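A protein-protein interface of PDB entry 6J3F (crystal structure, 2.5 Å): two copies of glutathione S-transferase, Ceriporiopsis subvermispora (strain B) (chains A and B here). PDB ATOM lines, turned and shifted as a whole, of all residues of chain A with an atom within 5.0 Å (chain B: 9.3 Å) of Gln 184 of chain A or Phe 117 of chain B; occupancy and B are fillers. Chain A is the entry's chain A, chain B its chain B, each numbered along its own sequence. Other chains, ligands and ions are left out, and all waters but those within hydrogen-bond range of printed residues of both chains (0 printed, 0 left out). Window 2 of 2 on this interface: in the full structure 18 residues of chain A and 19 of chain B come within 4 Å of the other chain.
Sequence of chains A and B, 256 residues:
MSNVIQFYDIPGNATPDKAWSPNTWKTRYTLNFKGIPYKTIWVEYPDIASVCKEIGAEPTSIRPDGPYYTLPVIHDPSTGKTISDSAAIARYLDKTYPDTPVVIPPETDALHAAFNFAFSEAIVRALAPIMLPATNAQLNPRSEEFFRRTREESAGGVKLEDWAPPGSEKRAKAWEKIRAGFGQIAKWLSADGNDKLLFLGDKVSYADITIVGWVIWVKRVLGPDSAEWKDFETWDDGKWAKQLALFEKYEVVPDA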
ATOM      1  N   ALA A 118      16.489   4.113 -19.495  1.00  0.00           N
ATOM      2  CA  ALA A 118      15.665   3.794 -20.661  1.00  0.00           C
ATOM      3  C   ALA A 118      15.765   2.322 -21.010  1.00  0.00           C
ATOM      4  O   ALA A 118      14.758   1.683 -21.338  1.00  0.00           O
ATOM      5  CB  ALA A 118      16.072   4.638 -21.863  1.00  0.00           C
ATOM      6  N   GLU A 121      13.937   0.015 -18.355  1.00  0.00           N
ATOM      7  CA  GLU A 121      12.500   0.098 -18.550  1.00  0.00           C
ATOM      8  C   GLU A 121      12.062  -0.638 -19.814  1.00  0.00           C
ATOM      9  O   GLU A 121      11.011  -1.285 -19.823  1.00  0.00           O
ATOM     10  CB  GLU A 121      12.078   1.568 -18.594  1.00  0.00           C
ATOM     11  CG  GLU A 121      12.155   2.251 -17.233  1.00  0.00           C
ATOM     12  CD  GLU A 121      11.390   1.464 -16.177  1.00  0.00           C
ATOM     13  OE1 GLU A 121      10.202   1.157 -16.420  1.00  0.00           O
ATOM     14  OE2 GLU A 121      11.991   1.131 -15.126  1.00  0.00           O
ATOM     15  N   ALA A 122      12.865  -0.577 -20.883  1.00  0.00           N
ATOM     16  CA  ALA A 122      12.407  -1.104 -22.162  1.00  0.00           C
ATOM     17  C   ALA A 122      12.684  -2.591 -22.304  1.00  0.00           C
ATOM     18  O   ALA A 122      11.918  -3.296 -22.960  1.00  0.00           O
ATOM     19  CB  ALA A 122      13.058  -0.339 -23.330  1.00  0.00           C
ATOM     20  N   ALA A 180       8.998  -5.888 -28.913  1.00  0.00           N
ATOM     21  CA  ALA A 180       8.718  -4.463 -29.009  1.00  0.00           C
ATOM     22  C   ALA A 180       9.749  -3.637 -28.237  1.00  0.00           C
ATOM     23  O   ALA A 180      10.124  -2.548 -28.686  1.00  0.00           O
ATOM     24  CB  ALA A 180       7.295  -4.181 -28.522  1.00  0.00           C
ATOM     25  N   GLY A 181      10.248  -4.152 -27.106  1.00  0.00           N
ATOM     26  CA  GLY A 181      11.289  -3.438 -26.371  1.00  0.00           C
ATOM     27  C   GLY A 181      12.549  -3.248 -27.193  1.00  0.00           C
ATOM     28  O   GLY A 181      13.114  -2.151 -27.254  1.00  0.00           O
ATOM     29  N   PHE A 182      13.001  -4.311 -27.858  1.00  0.00           N
ATOM     30  CA  PHE A 182      14.150  -4.156 -28.738  1.00  0.00           C
ATOM     31  C   PHE A 182      13.829  -3.295 -29.959  1.00  0.00           C
ATOM     32  O   PHE A 182      14.742  -2.689 -30.532  1.00  0.00           O
ATOM     33  CB  PHE A 182      14.676  -5.529 -29.150  1.00  0.00           C
ATOM     34  CG  PHE A 182      15.574  -6.141 -28.124  1.00  0.00           C
ATOM     35  CD1 PHE A 182      16.888  -5.725 -28.006  1.00  0.00           C
ATOM     36  CD2 PHE A 182      15.103  -7.105 -27.258  1.00  0.00           C
ATOM     37  CE1 PHE A 182      17.716  -6.262 -27.053  1.00  0.00           C
ATOM     38  CE2 PHE A 182      15.924  -7.649 -26.316  1.00  0.00           C
ATOM     39  CZ  PHE A 182      17.235  -7.226 -26.214  1.00  0.00           C
ATOM     40  N   GLY A 183      12.554  -3.211 -30.348  1.00  0.00           N
ATOM     41  CA  GLY A 183      12.177  -2.317 -31.427  1.00  0.00           C
ATOM     42  C   GLY A 183      12.467  -0.869 -31.096  1.00  0.00           C
ATOM     43  O   GLY A 183      12.859  -0.085 -31.968  1.00  0.00           O
ATOM     44  N   GLN A 184      12.306  -0.489 -29.833  1.00  0.00           N
ATOM     45  CA  GLN A 184      12.604   0.892 -29.502  1.00  0.00           C
ATOM     46  C   GLN A 184      14.092   1.167 -29.567  1.00  0.00           C
ATOM     47  O   GLN A 184      14.491   2.261 -29.976  1.00  0.00           O
ATOM     48  CB  GLN A 184      12.068   1.247 -28.133  1.00  0.00           C
ATOM     49  CG  GLN A 184      10.745   0.613 -27.843  1.00  0.00           C
ATOM     50  CD  GLN A 184      10.248   1.005 -26.476  1.00  0.00           C
ATOM     51  OE1 GLN A 184      10.390   2.159 -26.069  1.00  0.00           O
ATOM     52  NE2 GLN A 184       9.663   0.050 -25.750  1.00  0.00           N
ATOM     53  N   ILE A 185      14.933   0.198 -29.207  1.00  0.00           N
ATOM     54  CA  ILE A 185      16.365   0.427 -29.371  1.00  0.00           C
ATOM     55  C   ILE A 185      16.686   0.579 -30.846  1.00  0.00           C
ATOM     56  O   ILE A 185      17.458   1.462 -31.244  1.00  0.00           O
ATOM     57  CB  ILE A 185      17.186  -0.704 -28.732  1.00  0.00           C
ATOM     58  CG1 ILE A 185      16.801  -0.897 -27.272  1.00  0.00           C
ATOM     59  CG2 ILE A 185      18.673  -0.381 -28.827  1.00  0.00           C
ATOM     60  CD1 ILE A 185      17.801  -1.763 -26.494  1.00  0.00           C
ATOM     61  N   ALA A 186      16.077  -0.268 -31.682  1.00  0.00           N
ATOM     62  CA  ALA A 186      16.199  -0.103 -33.124  1.00  0.00           C
ATOM     63  C   ALA A 186      15.772   1.296 -33.561  1.00  0.00           C
ATOM     64  O   ALA A 186      16.441   1.916 -34.395  1.00  0.00           O
ATOM     65  CB  ALA A 186      15.381  -1.175 -33.849  1.00  0.00           C
ATOM     66  N   LYS A 187      14.670   1.822 -33.006  1.00  0.00           N
ATOM     67  CA  LYS A 187      14.274   3.190 -33.345  1.00  0.00           C
ATOM     68  C   LYS A 187      15.328   4.208 -32.890  1.00  0.00           C
ATOM     69  O   LYS A 187      15.654   5.145 -33.627  1.00  0.00           O
ATOM     70  CB  LYS A 187      12.907   3.519 -32.745  1.00  0.00           C
ATOM     71  CG  LYS A 187      12.701   5.021 -32.514  1.00  0.00           C
ATOM     72  CD  LYS A 187      11.754   5.355 -31.340  1.00  0.00           C
ATOM     73  CE  LYS A 187      10.302   5.569 -31.804  1.00  0.00           C
ATOM     74  NZ  LYS A 187       9.418   6.050 -30.685  1.00  0.00           N
ATOM     75  N   TRP A 188      15.894   4.030 -31.689  1.00  0.00           N
ATOM     76  CA  TRP A 188      16.884   4.993 -31.198  1.00  0.00           C
ATOM     77  C   TRP A 188      18.135   4.995 -32.067  1.00  0.00           C
ATOM     78  O   TRP A 188      18.699   6.058 -32.351  1.00  0.00           O
ATOM     79  CB  TRP A 188      17.282   4.694 -29.749  1.00  0.00           C
ATOM     80  CG  TRP A 188      16.146   4.508 -28.813  1.00  0.00           C
ATOM     81  CD1 TRP A 188      14.856   4.940 -28.980  1.00  0.00           C
ATOM     82  CD2 TRP A 188      16.183   3.824 -27.550  1.00  0.00           C
ATOM     83  NE1 TRP A 188      14.090   4.562 -27.896  1.00  0.00           N
ATOM     84  CE2 TRP A 188      14.880   3.881 -27.004  1.00  0.00           C
ATOM     85  CE3 TRP A 188      17.193   3.175 -26.823  1.00  0.00           C
ATOM     86  CZ2 TRP A 188      14.558   3.304 -25.761  1.00  0.00           C
ATOM     87  CZ3 TRP A 188      16.868   2.601 -25.584  1.00  0.00           C
ATOM     88  CH2 TRP A 188      15.564   2.675 -25.070  1.00  0.00           C
ATOM     89  N   ALA B  87      11.116  16.568 -31.487  1.00  0.00           N
ATOM     90  CA  ALA B  87      12.429  15.967 -31.726  1.00  0.00           C
ATOM     91  C   ALA B  87      12.767  15.961 -33.211  1.00  0.00           C
ATOM     92  O   ALA B  87      13.927  16.157 -33.590  1.00  0.00           O
ATOM     93  CB  ALA B  87      12.489  14.548 -31.164  1.00  0.00           C
ATOM     94  N   ALA B 110      21.576   9.022 -31.170  1.00  0.00           N
ATOM     95  CA  ALA B 110      20.908   7.829 -30.650  1.00  0.00           C
ATOM     96  C   ALA B 110      20.645   7.954 -29.152  1.00  0.00           C
ATOM     97  O   ALA B 110      19.531   7.676 -28.684  1.00  0.00           O
ATOM     98  CB  ALA B 110      21.738   6.583 -30.956  1.00  0.00           C
ATOM     99  N   LEU B 111      21.660   8.382 -28.386  1.00  0.00           N
ATOM    100  CA  LEU B 111      21.486   8.605 -26.951  1.00  0.00           C
ATOM    101  C   LEU B 111      20.405   9.640 -26.661  1.00  0.00           C
ATOM    102  O   LEU B 111      19.700   9.526 -25.655  1.00  0.00           O
ATOM    103  CB  LEU B 111      22.807   9.036 -26.304  1.00  0.00           C
ATOM    104  CG  LEU B 111      23.867   7.949 -26.022  1.00  0.00           C
ATOM    105  CD1 LEU B 111      25.253   8.555 -25.709  1.00  0.00           C
ATOM    106  CD2 LEU B 111      23.435   7.031 -24.892  1.00  0.00           C
ATOM    107  N   HIS B 112      20.249  10.652 -27.519  1.00  0.00           N
ATOM    108  CA  HIS B 112      19.125  11.574 -27.340  1.00  0.00           C
ATOM    109  C   HIS B 112      17.790  10.850 -27.524  1.00  0.00           C
ATOM    110  O   HIS B 112      16.808  11.149 -26.830  1.00  0.00           O
ATOM    111  CB  HIS B 112      19.239  12.756 -28.304  1.00  0.00           C
ATOM    112  CG  HIS B 112      19.944  13.957 -27.730  1.00  0.00           C
ATOM    113  ND1 HIS B 112      21.315  14.099 -27.748  1.00  0.00           N
ATOM    114  CD2 HIS B 112      19.459  15.086 -27.157  1.00  0.00           C
ATOM    115  CE1 HIS B 112      21.642  15.247 -27.188  1.00  0.00           C
ATOM    116  NE2 HIS B 112      20.535  15.869 -26.826  1.00  0.00           N
ATOM    117  N   ALA B 113      17.731   9.880 -28.441  1.00  0.00           N
ATOM    118  CA  ALA B 113      16.476   9.165 -28.637  1.00  0.00           C
ATOM    119  C   ALA B 113      16.204   8.221 -27.467  1.00  0.00           C
ATOM    120  O   ALA B 113      15.060   8.097 -27.019  1.00  0.00           O
ATOM    121  CB  ALA B 113      16.495   8.417 -29.972  1.00  0.00           C
ATOM    122  N   ALA B 114      17.246   7.573 -26.940  1.00  0.00           N
ATOM    123  CA  ALA B 114      17.108   6.857 -25.670  1.00  0.00           C
ATOM    124  C   ALA B 114      16.684   7.797 -24.547  1.00  0.00           C
ATOM    125  O   ALA B 114      15.883   7.421 -23.681  1.00  0.00           O
ATOM    126  CB  ALA B 114      18.418   6.160 -25.303  1.00  0.00           C
ATOM    127  N   PHE B 115      17.191   9.030 -24.552  1.00  0.00           N
ATOM    128  CA  PHE B 115      16.868   9.936 -23.454  1.00  0.00           C
ATOM    129  C   PHE B 115      15.398  10.321 -23.492  1.00  0.00           C
ATOM    130  O   PHE B 115      14.764  10.475 -22.442  1.00  0.00           O
ATOM    131  CB  PHE B 115      17.760  11.191 -23.482  1.00  0.00           C
ATOM    132  CG  PHE B 115      17.185  12.376 -22.709  1.00  0.00           C
ATOM    133  CD1 PHE B 115      17.476  12.554 -21.365  1.00  0.00           C
ATOM    134  CD2 PHE B 115      16.349  13.307 -23.335  1.00  0.00           C
ATOM    135  CE1 PHE B 115      16.950  13.638 -20.657  1.00  0.00           C
ATOM    136  CE2 PHE B 115      15.806  14.376 -22.627  1.00  0.00           C
ATOM    137  CZ  PHE B 115      16.117  14.545 -21.289  1.00  0.00           C
ATOM    138  N   ASN B 116      14.841  10.498 -24.692  1.00  0.00           N
ATOM    139  CA  ASN B 116      13.443  10.901 -24.767  1.00  0.00           C
ATOM    140  C   ASN B 116      12.527   9.819 -24.187  1.00  0.00           C
ATOM    141  O   ASN B 116      11.554  10.123 -23.487  1.00  0.00           O
ATOM    142  CB  ASN B 116      13.061  11.224 -26.201  1.00  0.00           C
ATOM    143  CG  ASN B 116      11.759  11.964 -26.276  1.00  0.00           C
ATOM    144  OD1 ASN B 116      11.432  12.785 -25.398  1.00  0.00           O
ATOM    145  ND2 ASN B 116      10.978  11.648 -27.271  1.00  0.00           N
ATOM    146  N   PHE B 117      12.831   8.550 -24.449  1.00  0.00           N
ATOM    147  CA  PHE B 117      12.059   7.477 -23.836  1.00  0.00           C
ATOM    148  C   PHE B 117      12.178   7.506 -22.312  1.00  0.00           C
ATOM    149  O   PHE B 117      11.164   7.575 -21.603  1.00  0.00           O
ATOM    150  CB  PHE B 117      12.505   6.129 -24.382  1.00  0.00           C
ATOM    151  CG  PHE B 117      11.781   4.978 -23.766  1.00  0.00           C
ATOM    152  CD1 PHE B 117      10.440   4.764 -24.047  1.00  0.00           C
ATOM    153  CD2 PHE B 117      12.436   4.113 -22.890  1.00  0.00           C
ATOM    154  CE1 PHE B 117       9.760   3.701 -23.462  1.00  0.00           C
ATOM    155  CE2 PHE B 117      11.763   3.044 -22.310  1.00  0.00           C
ATOM    156  CZ  PHE B 117      10.423   2.833 -22.598  1.00  0.00           C
ATOM    157  N   ALA B 118      13.417   7.440 -21.791  1.00  0.00           N
ATOM    158  CA  ALA B 118      13.639   7.474 -20.346  1.00  0.00           C
ATOM    159  C   ALA B 118      12.955   8.670 -19.710  1.00  0.00           C
ATOM    160  O   ALA B 118      12.450   8.574 -18.582  1.00  0.00           O
ATOM    161  CB  ALA B 118      15.145   7.517 -20.020  1.00  0.00           C
ATOM    162  N   PHE B 119      12.917   9.798 -20.427  1.00  0.00           N
ATOM    163  CA  PHE B 119      12.277  10.999 -19.908  1.00  0.00           C
ATOM    164  C   PHE B 119      10.751  10.849 -19.875  1.00  0.00           C
ATOM    165  O   PHE B 119      10.099  11.290 -18.920  1.00  0.00           O
ATOM    166  CB  PHE B 119      12.720  12.216 -20.750  1.00  0.00           C
ATOM    167  CG  PHE B 119      12.122  13.481 -20.296  1.00  0.00           C
ATOM    168  CD1 PHE B 119      12.735  14.214 -19.296  1.00  0.00           C
ATOM    169  CD2 PHE B 119      10.894  13.894 -20.800  1.00  0.00           C
ATOM    170  CE1 PHE B 119      12.156  15.365 -18.823  1.00  0.00           C
ATOM    171  CE2 PHE B 119      10.293  15.033 -20.344  1.00  0.00           C
ATOM    172  CZ  PHE B 119      10.927  15.788 -19.352  1.00  0.00           C
ATOM    173  N   SER B 120      10.166  10.223 -20.898  1.00  0.00           N
ATOM    174  CA  SER B 120       8.719   9.987 -20.923  1.00  0.00           C
ATOM    175  C   SER B 120       8.276   9.098 -19.770  1.00  0.00           C
ATOM    176  O   SER B 120       7.277   9.373 -19.097  1.00  0.00           O
ATOM    177  CB  SER B 120       8.328   9.340 -22.244  1.00  0.00           C
ATOM    178  OG  SER B 120       8.814  10.140 -23.305  1.00  0.00           O
ATOM    179  N   GLU B 121       8.985   7.992 -19.567  1.00  0.00           N
ATOM    180  CA  GLU B 121       8.677   7.108 -18.454  1.00  0.00           C
ATOM    181  C   GLU B 121       8.820   7.836 -17.124  1.00  0.00           C
ATOM    182  O   GLU B 121       7.859   7.953 -16.356  1.00  0.00           O
ATOM    183  CB  GLU B 121       9.586   5.886 -18.518  1.00  0.00           C
ATOM    184  CG  GLU B 121       9.283   4.999 -19.723  1.00  0.00           C
ATOM    185  CD  GLU B 121       7.789   4.723 -19.886  1.00  0.00           C
ATOM    186  OE1 GLU B 121       7.288   4.865 -21.014  1.00  0.00           O
ATOM    187  OE2 GLU B 121       7.115   4.375 -18.886  1.00  0.00           O
ATOM    188  N   ALA B 122      10.005   8.394 -16.863  1.00  0.00           N
ATOM    189  CA  ALA B 122      10.259   8.963 -15.550  1.00  0.00           C
ATOM    190  C   ALA B 122       9.452  10.226 -15.289  1.00  0.00           C
ATOM    191  O   ALA B 122       9.154  10.516 -14.134  1.00  0.00           O
ATOM    192  CB  ALA B 122      11.751   9.248 -15.386  1.00  0.00           C
ATOM    193  N   ILE B 123       9.108  11.010 -16.314  1.00  0.00           N
ATOM    194  CA  ILE B 123       8.567  12.350 -16.051  1.00  0.00           C
ATOM    195  C   ILE B 123       7.145  12.535 -16.583  1.00  0.00           C
ATOM    196  O   ILE B 123       6.220  12.848 -15.819  1.00  0.00           O
ATOM    197  CB  ILE B 123       9.493  13.437 -16.630  1.00  0.00           C
ATOM    198  CG1 ILE B 123      10.925  13.253 -16.109  1.00  0.00           C
ATOM    199  CG2 ILE B 123       8.922  14.851 -16.362  1.00  0.00           C
ATOM    200  CD1 ILE B 123      11.111  13.460 -14.625  1.00  0.00           C
ATOM    201  N   VAL B 124       6.962  12.371 -17.897  1.00  0.00           N
ATOM    202  CA  VAL B 124       5.669  12.677 -18.514  1.00  0.00           C
ATOM    203  C   VAL B 124       4.560  11.854 -17.877  1.00  0.00           C
ATOM    204  O   VAL B 124       3.469  12.363 -17.577  1.00  0.00           O
ATOM    205  CB  VAL B 124       5.727  12.441 -20.031  1.00  0.00           C
ATOM    206  CG1 VAL B 124       4.380  12.806 -20.661  1.00  0.00           C
ATOM    207  CG2 VAL B 124       6.895  13.239 -20.639  1.00  0.00           C
ATOM    208  N   ARG B 125       4.813  10.569 -17.668  1.00  0.00           N
ATOM    209  CA  ARG B 125       3.774   9.717 -17.108  1.00  0.00           C
ATOM    210  C   ARG B 125       3.413  10.157 -15.687  1.00  0.00           C
ATOM    211  O   ARG B 125       2.233  10.180 -15.313  1.00  0.00           O
ATOM    212  CB  ARG B 125       4.233   8.261 -17.163  1.00  0.00           C
ATOM    213  CG  ARG B 125       3.077   7.269 -17.182  1.00  0.00           C
ATOM    214  CD  ARG B 125       3.571   5.836 -17.095  1.00  0.00           C
ATOM    215  NE  ARG B 125       4.405   5.481 -18.236  1.00  0.00           N
ATOM    216  CZ  ARG B 125       3.934   5.283 -19.466  1.00  0.00           C
ATOM    217  NH1 ARG B 125       2.633   5.417 -19.717  1.00  0.00           N
ATOM    218  NH2 ARG B 125       4.764   4.958 -20.451  1.00  0.00           N
ATOM    219  N   TRP B 188      21.291  11.295 -13.020  1.00  0.00           N
ATOM    220  CA  TRP B 188      21.918  11.193 -14.336  1.00  0.00           C
ATOM    221  C   TRP B 188      22.906  12.321 -14.552  1.00  0.00           C
ATOM    222  O   TRP B 188      23.979  12.117 -15.125  1.00  0.00           O
ATOM    223  CB  TRP B 188      20.874  11.219 -15.455  1.00  0.00           C
ATOM    224  CG  TRP B 188      19.790  10.206 -15.342  1.00  0.00           C
ATOM    225  CD1 TRP B 188      19.781   9.080 -14.565  1.00  0.00           C
ATOM    226  CD2 TRP B 188      18.528  10.246 -16.013  1.00  0.00           C
ATOM    227  NE1 TRP B 188      18.592   8.416 -14.719  1.00  0.00           N
ATOM    228  CE2 TRP B 188      17.805   9.110 -15.604  1.00  0.00           C
ATOM    229  CE3 TRP B 188      17.942  11.131 -16.933  1.00  0.00           C
ATOM    230  CZ2 TRP B 188      16.523   8.835 -16.076  1.00  0.00           C
ATOM    231  CZ3 TRP B 188      16.668  10.853 -17.407  1.00  0.00           C
ATOM    232  CH2 TRP B 188      15.969   9.724 -16.965  1.00  0.00           C
ATOM    233  N   THR B 210      14.481  19.715 -23.648  1.00  0.00           N
ATOM    234  CA  THR B 210      13.374  18.837 -23.275  1.00  0.00           C
ATOM    235  C   THR B 210      12.918  19.094 -21.841  1.00  0.00           C
ATOM    236  O   THR B 210      11.717  19.263 -21.585  1.00  0.00           O
ATOM    237  CB  THR B 210      13.784  17.377 -23.464  1.00  0.00           C
ATOM    238  OG1 THR B 210      14.105  17.156 -24.845  1.00  0.00           O
ATOM    239  CG2 THR B 210      12.644  16.428 -23.032  1.00  0.00           C
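The indole nitrogen (NE1) of Trp 188 of chain A sits close to the backbone carbonyl oxygen (O) of Gln 184 of chain A (3.1 Å).
CB of Ala 118 of chain A touches O of Ala 114 of chain B, at 3.3 Å.
CE2 of Phe 117 of chain B touches O of Ala 118 of chain A (3.4 Å).
Ala 118 of chain B touches Ala 118 of chain A (CB to CB, 3.5 Å).
Phe 117 of chain B touches Ala 122 of chain A (CE2 to CB, 3.8 Å).
Phe 117 of chain B touches Gln 184 of chain A (CE1 to OE1, 3.1 Å).
Ala 110 of chain B touches Trp 188 of chain A (CA to O, 3.3 Å).
CB of Ala 113 of chain B touches CA of Trp 188 of chain A (3.7 Å).
CB of Ala 114 of chain B touches CE3 of Trp 188 of chain A, at 3.6 Å.
CD2 of Phe 117 of chain B touches CZ2 of Trp 188 of chain A, 3.7 Å away.
No residue of chain B comes within 4 Å of Gly 183 of chain A.
Of chain B, only Phe 117 comes within 4 Å of Gln 184 of chain A.
Of the printed residues of chain A, Ala 113 of chain B touches Trp 188 (3.7 Å).
Of the printed residues of chain A, Ala 114 of chain B touches Ala 118 (3.3 Å) and Trp 188 (3.6 Å).
Of the printed residues of chain A, Ala 118 of chain B touches Ala 118 (3.5 Å).
Ala 122 of chain B touches none of the printed residues of chain A.
Arg 125 of chain B touches none of the printed residues of chain A.
The nearest printed residue of chain B that does not touch Ala 122 of chain A is Glu 121 of chain B (6.7 Å).
Hydrophobic or aromatic side chains of chain A that line the printed part of chain B: Ala 118, Ala 122 and Trp 188.
Hydrophobic or aromatic side chains of chain B within 4 Å of the printed part of chain A: Ala 110, Ala 113, Ala 114, Phe 117 and Ala 118.
Along chain B the printed residues that touch a printed residue of chain A span positions 110 to 118.
Among the printed residues, 9 pairs touch across the chains.
Among the printed residues, no Asp or Glu carboxylate lies within 4 Å of a Lys or Arg side-chain nitrogen of the other chain.
Ala 118 of chain B touches its own counterpart, Ala 118 of chain A.
Positions printed for both chains: 118, 121, 122 and 188.
Of the 9 pairs that touch across the chains among the printed residues, 1 has its exchanged pair printed and touching as well.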
